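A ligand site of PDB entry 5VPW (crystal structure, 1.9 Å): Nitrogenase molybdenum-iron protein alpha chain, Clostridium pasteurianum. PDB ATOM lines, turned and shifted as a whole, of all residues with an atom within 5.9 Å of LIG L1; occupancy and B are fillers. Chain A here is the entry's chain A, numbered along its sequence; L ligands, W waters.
The side-chain sulfur of Cys 262 is bound to an iron atom (FE1) of LIG L1.
A ring nitrogen (ND1) of His 482 is bound to a molybdenum atom (MO1) of LIG L1, 2.4 Å away.
NE2 of His 186 lies close to S4 of LIG L1 (3.2 Å).
The backbone NH of Gly 344 sits close to a sulfur (S5) of LIG L1 (3.3 Å).
The guanidinium group of Arg 87 sits close to a sulfur (S6) of LIG L1, at 3.3 Å.
A sulfur (S5) of LIG L1 lies close to the guanidinium group (NH1) of Arg 347 (3.3 Å).
N of Gly 345 sits close to S5 of LIG L1.
The side-chain hydroxyl (OG) of Ser 265 lies close to a sulfur (S3) of LIG L1, at 3.6 Å.
NE2 of Gln 182 sits at hydrogen-bond distance from O2 of LG2 L2 (2.9 Å).
An oxygen (O7) of LG2 L2 binds a molybdenum atom (MO1) of LIG L1 (2.1 Å).
OG of Ser 265 lies close to SG of Cys 262, 3.3 Å away.
The side-chain sulfur (SG) of Cys 262 sits close to the backbone NH (N) of Arg 264 (3.7 Å).
O of Gly 214 sits at hydrogen-bond distance from N of Cys 262, 3.0 Å away.
O of Gly 344 sits at hydrogen-bond distance from N of Phe 369 (3.1 Å).
The backbone NH (N) of Glu 368 sits at hydrogen-bond distance from the backbone carbonyl oxygen (O) of Gly 344 (3.0 Å).
NH2 of Arg 87 is in hydrogen-bond range of O of Val 61 (2.8 Å).
The backbone carbonyl oxygen (O) of Leu 481 lies within hydrogen-bond range of the guanidinium group (NH2) of Arg 347, 2.7 Å away.
OG of Ser 265 is in hydrogen-bond range of OH of Tyr 216, at 2.8 Å.
The backbone carbonyl oxygen (O) of Ser 346 lies close to a sulfur (S5) of LIG L1, 3.8 Å away.
Residues that only touch LIG L1: Phe 369 (3.5 Å), Tyr 216 (3.6 Å) and Val 61 (3.6 Å).
Hydrophobic or aromatic side chains that line LIG L1: Val 61, His 186, Tyr 216, Phe 369 and His 482.
Of the 21 residues printed, 12 come within 4 Å of LIG L1.
The nearest printed residue that does not touch LIG L1 is Ile 218 (4.05 Å).
Water W1 lies within hydrogen-bond range of the backbone carbonyl oxygen of Gly 214 (2.7 Å) and a sulfur (S7) of LIG L1 (3.4 Å).
Water W2 lies within hydrogen-bond range of O of His 482 (2.8 Å) and S8 of LIG L1 (3.5 Å).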
ATOM      1  N   GLY A  57      -0.174 -25.556  -9.999  1.00  0.00           N
ATOM      2  CA  GLY A  57       1.254 -25.881  -9.942  1.00  0.00           C
ATOM      3  C   GLY A  57       2.121 -24.953 -10.788  1.00  0.00           C
ATOM      4  O   GLY A  57       3.249 -24.608 -10.401  1.00  0.00           O
ATOM      5  N   VAL A  61       2.150 -21.573  -8.315  1.00  0.00           N
ATOM      6  CA  VAL A  61       3.293 -22.026  -7.512  1.00  0.00           C
ATOM      7  C   VAL A  61       4.648 -21.611  -8.059  1.00  0.00           C
ATOM      8  O   VAL A  61       5.347 -20.786  -7.445  1.00  0.00           O
ATOM      9  CB  VAL A  61       3.221 -23.570  -7.291  1.00  0.00           C
ATOM     10  CG1 VAL A  61       4.435 -24.061  -6.532  1.00  0.00           C
ATOM     11  CG2 VAL A  61       1.956 -23.911  -6.510  1.00  0.00           C
ATOM     12  N   ARG A  87      -1.469 -17.689  -1.613  1.00  0.00           N
ATOM     13  CA  ARG A  87      -0.165 -18.290  -1.402  1.00  0.00           C
ATOM     14  C   ARG A  87       0.806 -17.129  -1.085  1.00  0.00           C
ATOM     15  O   ARG A  87       0.916 -16.206  -1.877  1.00  0.00           O
ATOM     16  CB  ARG A  87       0.299 -19.056  -2.631  1.00  0.00           C
ATOM     17  CG  ARG A  87       1.661 -19.757  -2.388  1.00  0.00           C
ATOM     18  CD  ARG A  87       1.885 -20.891  -3.381  1.00  0.00           C
ATOM     19  NE  ARG A  87       3.264 -21.431  -3.393  1.00  0.00           N
ATOM     20  CZ  ARG A  87       4.236 -20.984  -4.175  1.00  0.00           C
ATOM     21  NH1 ARG A  87       5.432 -21.587  -4.145  1.00  0.00           N
ATOM     22  NH2 ARG A  87       4.017 -20.010  -5.050  1.00  0.00           N
ATOM     23  N   GLN A 182      -0.899 -30.843  -8.778  1.00  0.00           N
ATOM     24  CA  GLN A 182      -0.025 -29.671  -9.010  1.00  0.00           C
ATOM     25  C   GLN A 182       1.268 -30.009  -9.709  1.00  0.00           C
ATOM     26  O   GLN A 182       1.850 -29.151 -10.375  1.00  0.00           O
ATOM     27  CB  GLN A 182       0.340 -28.975  -7.673  1.00  0.00           C
ATOM     28  CG  GLN A 182      -0.807 -28.336  -6.923  1.00  0.00           C
ATOM     29  CD  GLN A 182      -1.471 -29.265  -5.909  1.00  0.00           C
ATOM     30  OE1 GLN A 182      -1.793 -30.412  -6.191  1.00  0.00           O
ATOM     31  NE2 GLN A 182      -1.695 -28.748  -4.721  1.00  0.00           N
ATOM     32  N   HIS A 186       4.244 -27.937 -12.165  1.00  0.00           N
ATOM     33  CA  HIS A 186       5.656 -27.681 -11.973  1.00  0.00           C
ATOM     34  C   HIS A 186       6.457 -28.049 -13.199  1.00  0.00           C
ATOM     35  O   HIS A 186       7.288 -27.259 -13.681  1.00  0.00           O
ATOM     36  CB  HIS A 186       6.227 -28.498 -10.823  1.00  0.00           C
ATOM     37  CG  HIS A 186       5.503 -28.361  -9.522  1.00  0.00           C
ATOM     38  ND1 HIS A 186       5.532 -29.335  -8.547  1.00  0.00           N
ATOM     39  CD2 HIS A 186       4.724 -27.360  -9.036  1.00  0.00           C
ATOM     40  CE1 HIS A 186       4.789 -28.954  -7.528  1.00  0.00           C
ATOM     41  NE2 HIS A 186       4.292 -27.757  -7.789  1.00  0.00           N
ATOM     42  N   GLY A 214      13.782 -23.974  -6.115  1.00  0.00           N
ATOM     43  CA  GLY A 214      12.583 -24.583  -5.496  1.00  0.00           C
ATOM     44  C   GLY A 214      12.303 -23.977  -4.140  1.00  0.00           C
ATOM     45  O   GLY A 214      12.018 -24.679  -3.150  1.00  0.00           O
ATOM     46  N   TYR A 216      10.308 -20.441  -2.590  1.00  0.00           N
ATOM     47  CA  TYR A 216       9.322 -19.447  -3.043  1.00  0.00           C
ATOM     48  C   TYR A 216       9.079 -18.321  -2.043  1.00  0.00           C
ATOM     49  O   TYR A 216       8.190 -17.535  -2.240  1.00  0.00           O
ATOM     50  CB  TYR A 216       8.031 -20.183  -3.477  1.00  0.00           C
ATOM     51  CG  TYR A 216       8.382 -21.258  -4.499  1.00  0.00           C
ATOM     52  CD1 TYR A 216       8.669 -20.928  -5.815  1.00  0.00           C
ATOM     53  CD2 TYR A 216       8.471 -22.598  -4.128  1.00  0.00           C
ATOM     54  CE1 TYR A 216       9.053 -21.890  -6.725  1.00  0.00           C
ATOM     55  CE2 TYR A 216       8.866 -23.582  -5.039  1.00  0.00           C
ATOM     56  CZ  TYR A 216       9.123 -23.226  -6.343  1.00  0.00           C
ATOM     57  OH  TYR A 216       9.495 -24.166  -7.275  1.00  0.00           O
ATOM     58  N   ILE A 218       8.046 -18.131   0.981  1.00  0.00           N
ATOM     59  CA  ILE A 218       6.765 -18.068   1.679  1.00  0.00           C
ATOM     60  C   ILE A 218       7.037 -17.447   3.047  1.00  0.00           C
ATOM     61  O   ILE A 218       7.880 -17.937   3.807  1.00  0.00           O
ATOM     62  CB  ILE A 218       6.105 -19.457   1.822  1.00  0.00           C
ATOM     63  CG1 ILE A 218       5.994 -20.124   0.456  1.00  0.00           C
ATOM     64  CG2 ILE A 218       4.759 -19.375   2.557  1.00  0.00           C
ATOM     65  CD1 ILE A 218       5.204 -19.348  -0.582  1.00  0.00           C
ATOM     66  N   CYS A 262      12.959 -27.511  -2.697  1.00  0.00           N
ATOM     67  CA  CYS A 262      11.927 -28.396  -3.185  1.00  0.00           C
ATOM     68  C   CYS A 262      12.348 -29.241  -4.374  1.00  0.00           C
ATOM     69  O   CYS A 262      12.290 -28.760  -5.526  1.00  0.00           O
ATOM     70  CB  CYS A 262      10.632 -27.664  -3.623  1.00  0.00           C
ATOM     71  SG  CYS A 262       9.306 -28.865  -3.970  1.00  0.00           S
ATOM     72  N   ARG A 264      10.617 -31.860  -5.603  1.00  0.00           N
ATOM     73  CA  ARG A 264       9.482 -32.159  -6.465  1.00  0.00           C
ATOM     74  C   ARG A 264       9.292 -31.096  -7.555  1.00  0.00           C
ATOM     75  O   ARG A 264       9.128 -31.439  -8.748  1.00  0.00           O
ATOM     76  CB  ARG A 264       8.208 -32.289  -5.625  1.00  0.00           C
ATOM     77  CG  ARG A 264       6.945 -32.523  -6.407  1.00  0.00           C
ATOM     78  CD  ARG A 264       6.919 -33.913  -7.008  1.00  0.00           C
ATOM     79  NE  ARG A 264       7.376 -33.921  -8.407  1.00  0.00           N
ATOM     80  CZ  ARG A 264       8.328 -34.715  -8.898  1.00  0.00           C
ATOM     81  NH1 ARG A 264       8.970 -35.583  -8.106  1.00  0.00           N
ATOM     82  NH2 ARG A 264       8.648 -34.622 -10.189  1.00  0.00           N
ATOM     83  N   SER A 265       9.326 -29.811  -7.163  1.00  0.00           N
ATOM     84  CA  SER A 265       8.906 -28.746  -8.065  1.00  0.00           C
ATOM     85  C   SER A 265       9.981 -28.284  -9.017  1.00  0.00           C
ATOM     86  O   SER A 265       9.636 -27.728 -10.023  1.00  0.00           O
ATOM     87  CB  SER A 265       8.351 -27.506  -7.308  1.00  0.00           C
ATOM     88  OG  SER A 265       9.314 -26.816  -6.551  1.00  0.00           O
ATOM     89  N   VAL A 343       1.405 -32.829   4.066  1.00  0.00           N
ATOM     90  CA  VAL A 343       2.024 -31.837   3.184  1.00  0.00           C
ATOM     91  C   VAL A 343       1.605 -32.034   1.744  1.00  0.00           C
ATOM     92  O   VAL A 343       0.895 -32.996   1.426  1.00  0.00           O
ATOM     93  CB  VAL A 343       3.559 -31.962   3.243  1.00  0.00           C
ATOM     94  CG1 VAL A 343       4.067 -31.697   4.675  1.00  0.00           C
ATOM     95  CG2 VAL A 343       4.037 -33.339   2.755  1.00  0.00           C
ATOM     96  N   GLY A 344       2.053 -31.145   0.864  1.00  0.00           N
ATOM     97  CA  GLY A 344       1.841 -31.348  -0.583  1.00  0.00           C
ATOM     98  C   GLY A 344       2.752 -32.393  -1.191  1.00  0.00           C
ATOM     99  O   GLY A 344       2.319 -33.497  -1.466  1.00  0.00           O
ATOM    100  N   GLY A 345       4.024 -32.060  -1.358  1.00  0.00           N
ATOM    101  CA  GLY A 345       4.995 -32.890  -2.087  1.00  0.00           C
ATOM    102  C   GLY A 345       6.405 -32.880  -1.536  1.00  0.00           C
ATOM    103  O   GLY A 345       7.296 -33.471  -2.128  1.00  0.00           O
ATOM    104  N   SER A 346       6.627 -32.184  -0.408  1.00  0.00           N
ATOM    105  CA  SER A 346       7.964 -31.968   0.104  1.00  0.00           C
ATOM    106  C   SER A 346       7.884 -31.655   1.607  1.00  0.00           C
ATOM    107  O   SER A 346       6.797 -31.390   2.131  1.00  0.00           O
ATOM    108  CB  SER A 346       8.586 -30.783  -0.660  1.00  0.00           C
ATOM    109  OG  SER A 346       9.888 -30.415  -0.256  1.00  0.00           O
ATOM    110  N   ARG A 347       9.050 -31.612   2.248  1.00  0.00           N
ATOM    111  CA  ARG A 347       9.258 -31.071   3.586  1.00  0.00           C
ATOM    112  C   ARG A 347       8.877 -31.993   4.758  1.00  0.00           C
ATOM    113  O   ARG A 347       9.042 -31.616   5.891  1.00  0.00           O
ATOM    114  CB  ARG A 347       8.513 -29.705   3.736  1.00  0.00           C
ATOM    115  CG  ARG A 347       8.922 -28.651   2.686  1.00  0.00           C
ATOM    116  CD  ARG A 347       8.091 -27.360   2.795  1.00  0.00           C
ATOM    117  NE  ARG A 347       6.669 -27.664   2.708  1.00  0.00           N
ATOM    118  CZ  ARG A 347       5.715 -27.037   3.398  1.00  0.00           C
ATOM    119  NH1 ARG A 347       4.449 -27.402   3.242  1.00  0.00           N
ATOM    120  NH2 ARG A 347       6.021 -26.066   4.242  1.00  0.00           N
ATOM    121  N   GLU A 368      -0.121 -35.050  -0.555  1.00  0.00           N
ATOM    122  CA  GLU A 368      -1.060 -34.851  -1.661  1.00  0.00           C
ATOM    123  C   GLU A 368      -0.572 -35.560  -2.907  1.00  0.00           C
ATOM    124  O   GLU A 368      -1.329 -36.336  -3.535  1.00  0.00           O
ATOM    125  CB  GLU A 368      -1.251 -33.379  -1.978  1.00  0.00           C
ATOM    126  CG  GLU A 368      -1.948 -32.608  -0.879  1.00  0.00           C
ATOM    127  CD  GLU A 368      -2.325 -31.177  -1.225  1.00  0.00           C
ATOM    128  OE1 GLU A 368      -2.598 -30.449  -0.234  1.00  0.00           O
ATOM    129  OE2 GLU A 368      -2.404 -30.800  -2.423  1.00  0.00           O
ATOM    130  N   PHE A 369       0.664 -35.307  -3.289  1.00  0.00           N
ATOM    131  CA  PHE A 369       1.081 -35.609  -4.671  1.00  0.00           C
ATOM    132  C   PHE A 369       2.542 -35.921  -4.913  1.00  0.00           C
ATOM    133  O   PHE A 369       2.992 -35.824  -6.080  1.00  0.00           O
ATOM    134  CB  PHE A 369       0.699 -34.446  -5.582  1.00  0.00           C
ATOM    135  CG  PHE A 369       1.284 -33.143  -5.165  1.00  0.00           C
ATOM    136  CD1 PHE A 369       2.632 -32.864  -5.350  1.00  0.00           C
ATOM    137  CD2 PHE A 369       0.486 -32.220  -4.545  1.00  0.00           C
ATOM    138  CE1 PHE A 369       3.142 -31.654  -4.917  1.00  0.00           C
ATOM    139  CE2 PHE A 369       0.996 -31.011  -4.113  1.00  0.00           C
ATOM    140  CZ  PHE A 369       2.313 -30.733  -4.318  1.00  0.00           C
ATOM    141  N   LEU A 481       0.946 -25.857   7.505  1.00  0.00           N
ATOM    142  CA  LEU A 481       2.286 -25.972   6.946  1.00  0.00           C
ATOM    143  C   LEU A 481       2.462 -25.310   5.615  1.00  0.00           C
ATOM    144  O   LEU A 481       3.603 -25.222   5.122  1.00  0.00           O
ATOM    145  CB  LEU A 481       2.662 -27.457   6.804  1.00  0.00           C
ATOM    146  CG  LEU A 481       2.769 -28.234   8.092  1.00  0.00           C
ATOM    147  CD1 LEU A 481       3.255 -29.648   7.865  1.00  0.00           C
ATOM    148  CD2 LEU A 481       3.707 -27.532   9.049  1.00  0.00           C
ATOM    149  N   HIS A 482       1.388 -24.823   4.985  1.00  0.00           N
ATOM    150  CA  HIS A 482       1.542 -24.106   3.763  1.00  0.00           C
ATOM    151  C   HIS A 482       1.603 -22.590   4.032  1.00  0.00           C
ATOM    152  O   HIS A 482       2.619 -21.942   3.741  1.00  0.00           O
ATOM    153  CB  HIS A 482       0.445 -24.348   2.717  1.00  0.00           C
ATOM    154  CG  HIS A 482       0.076 -25.770   2.461  1.00  0.00           C
ATOM    155  ND1 HIS A 482       0.173 -26.355   1.208  1.00  0.00           N
ATOM    156  CD2 HIS A 482      -0.467 -26.716   3.264  1.00  0.00           C
ATOM    157  CE1 HIS A 482      -0.313 -27.585   1.262  1.00  0.00           C
ATOM    158  NE2 HIS A 482      -0.695 -27.827   2.489  1.00  0.00           N
ATOM    159  N   SER A 483       0.514 -22.033   4.569  1.00  0.00           N
ATOM    160  CA  SER A 483       0.435 -20.592   4.868  1.00  0.00           C
ATOM    161  C   SER A 483       1.155 -20.152   6.142  1.00  0.00           C
ATOM    162  O   SER A 483       1.257 -18.937   6.399  1.00  0.00           O
ATOM    163  CB  SER A 483      -1.045 -20.192   5.020  1.00  0.00           C
ATOM    164  OG  SER A 483      -1.616 -20.779   6.191  1.00  0.00           O
HETATM  165 FE1  LIG L   1       7.403 -27.885  -3.276  1.00  0.00          FE
HETATM  166 MO1  LIG L   1       1.280 -25.570  -0.771  1.00  0.00          MO
HETATM  167 FE2  LIG L   1       4.786 -27.505  -3.816  1.00  0.00          FE
HETATM  168 FE3  LIG L   1       6.109 -25.741  -2.312  1.00  0.00          FE
HETATM  169 FE4  LIG L   1       5.545 -28.191  -1.391  1.00  0.00          FE
HETATM  170 FE5  LIG L   1       3.240 -27.335  -0.479  1.00  0.00          FE
HETATM  171 FE6  LIG L   1       2.569 -26.604  -2.885  1.00  0.00          FE
HETATM  172 FE7  LIG L   1       3.818 -24.920  -1.360  1.00  0.00          FE
HETATM  173  C1  LIG L   1       4.389 -26.760  -2.004  1.00  0.00           C
HETATM  174  S1  LIG L   1       5.783 -29.488  -3.235  1.00  0.00           S
HETATM  175  S2  LIG L   1       1.296 -27.802  -1.545  1.00  0.00           S
HETATM  176  S3  LIG L   1       6.479 -26.189  -4.499  1.00  0.00           S
HETATM  177  S4  LIG L   1       2.862 -27.344  -4.922  1.00  0.00           S
HETATM  178  S5  LIG L   1       4.474 -28.987   0.361  1.00  0.00           S
HETATM  179  S6  LIG L   1       2.066 -24.412  -2.701  1.00  0.00           S
HETATM  180  S7  LIG L   1       7.500 -27.023  -1.140  1.00  0.00           S
HETATM  181  S8  LIG L   1       3.139 -25.430   0.725  1.00  0.00           S
HETATM  182  S9  LIG L   1       5.569 -23.614  -1.545  1.00  0.00           S
HETATM  183  C1  LG2 L   2      -1.931 -24.836  -3.977  1.00  0.00           C
HETATM  184  C2  LG2 L   2      -1.460 -23.713  -3.082  1.00  0.00           C
HETATM  185  C3  LG2 L   2      -1.329 -24.179  -1.626  1.00  0.00           C
HETATM  186  C4  LG2 L   2      -2.656 -24.296  -0.871  1.00  0.00           C
HETATM  187  C5  LG2 L   2      -2.425 -24.365   0.664  1.00  0.00           C
HETATM  188  C6  LG2 L   2      -3.545 -24.969   1.524  1.00  0.00           C
HETATM  189  C7  LG2 L   2      -0.498 -23.150  -0.861  1.00  0.00           C
HETATM  190  O1  LG2 L   2      -2.622 -24.538  -4.983  1.00  0.00           O
HETATM  191  O2  LG2 L   2      -1.575 -26.005  -3.711  1.00  0.00           O
HETATM  192  O3  LG2 L   2      -3.678 -24.480   2.683  1.00  0.00           O
HETATM  193  O4  LG2 L   2      -4.268 -25.904   1.094  1.00  0.00           O
HETATM  194  O5  LG2 L   2      -0.900 -21.996  -0.823  1.00  0.00           O
HETATM  195  O6  LG2 L   2       0.496 -23.500  -0.195  1.00  0.00           O
HETATM  196  O7  LG2 L   2      -0.645 -25.441  -1.634  1.00  0.00           O
HETATM  197  O   HOH W   1      10.121 -24.832  -1.256  1.00  0.00           O
HETATM  198  O   HOH W   2       4.870 -23.049   2.591  1.00  0.00           O
HETATM  199  O   HOH W   3       7.094 -23.855   1.594  1.00  0.00           O
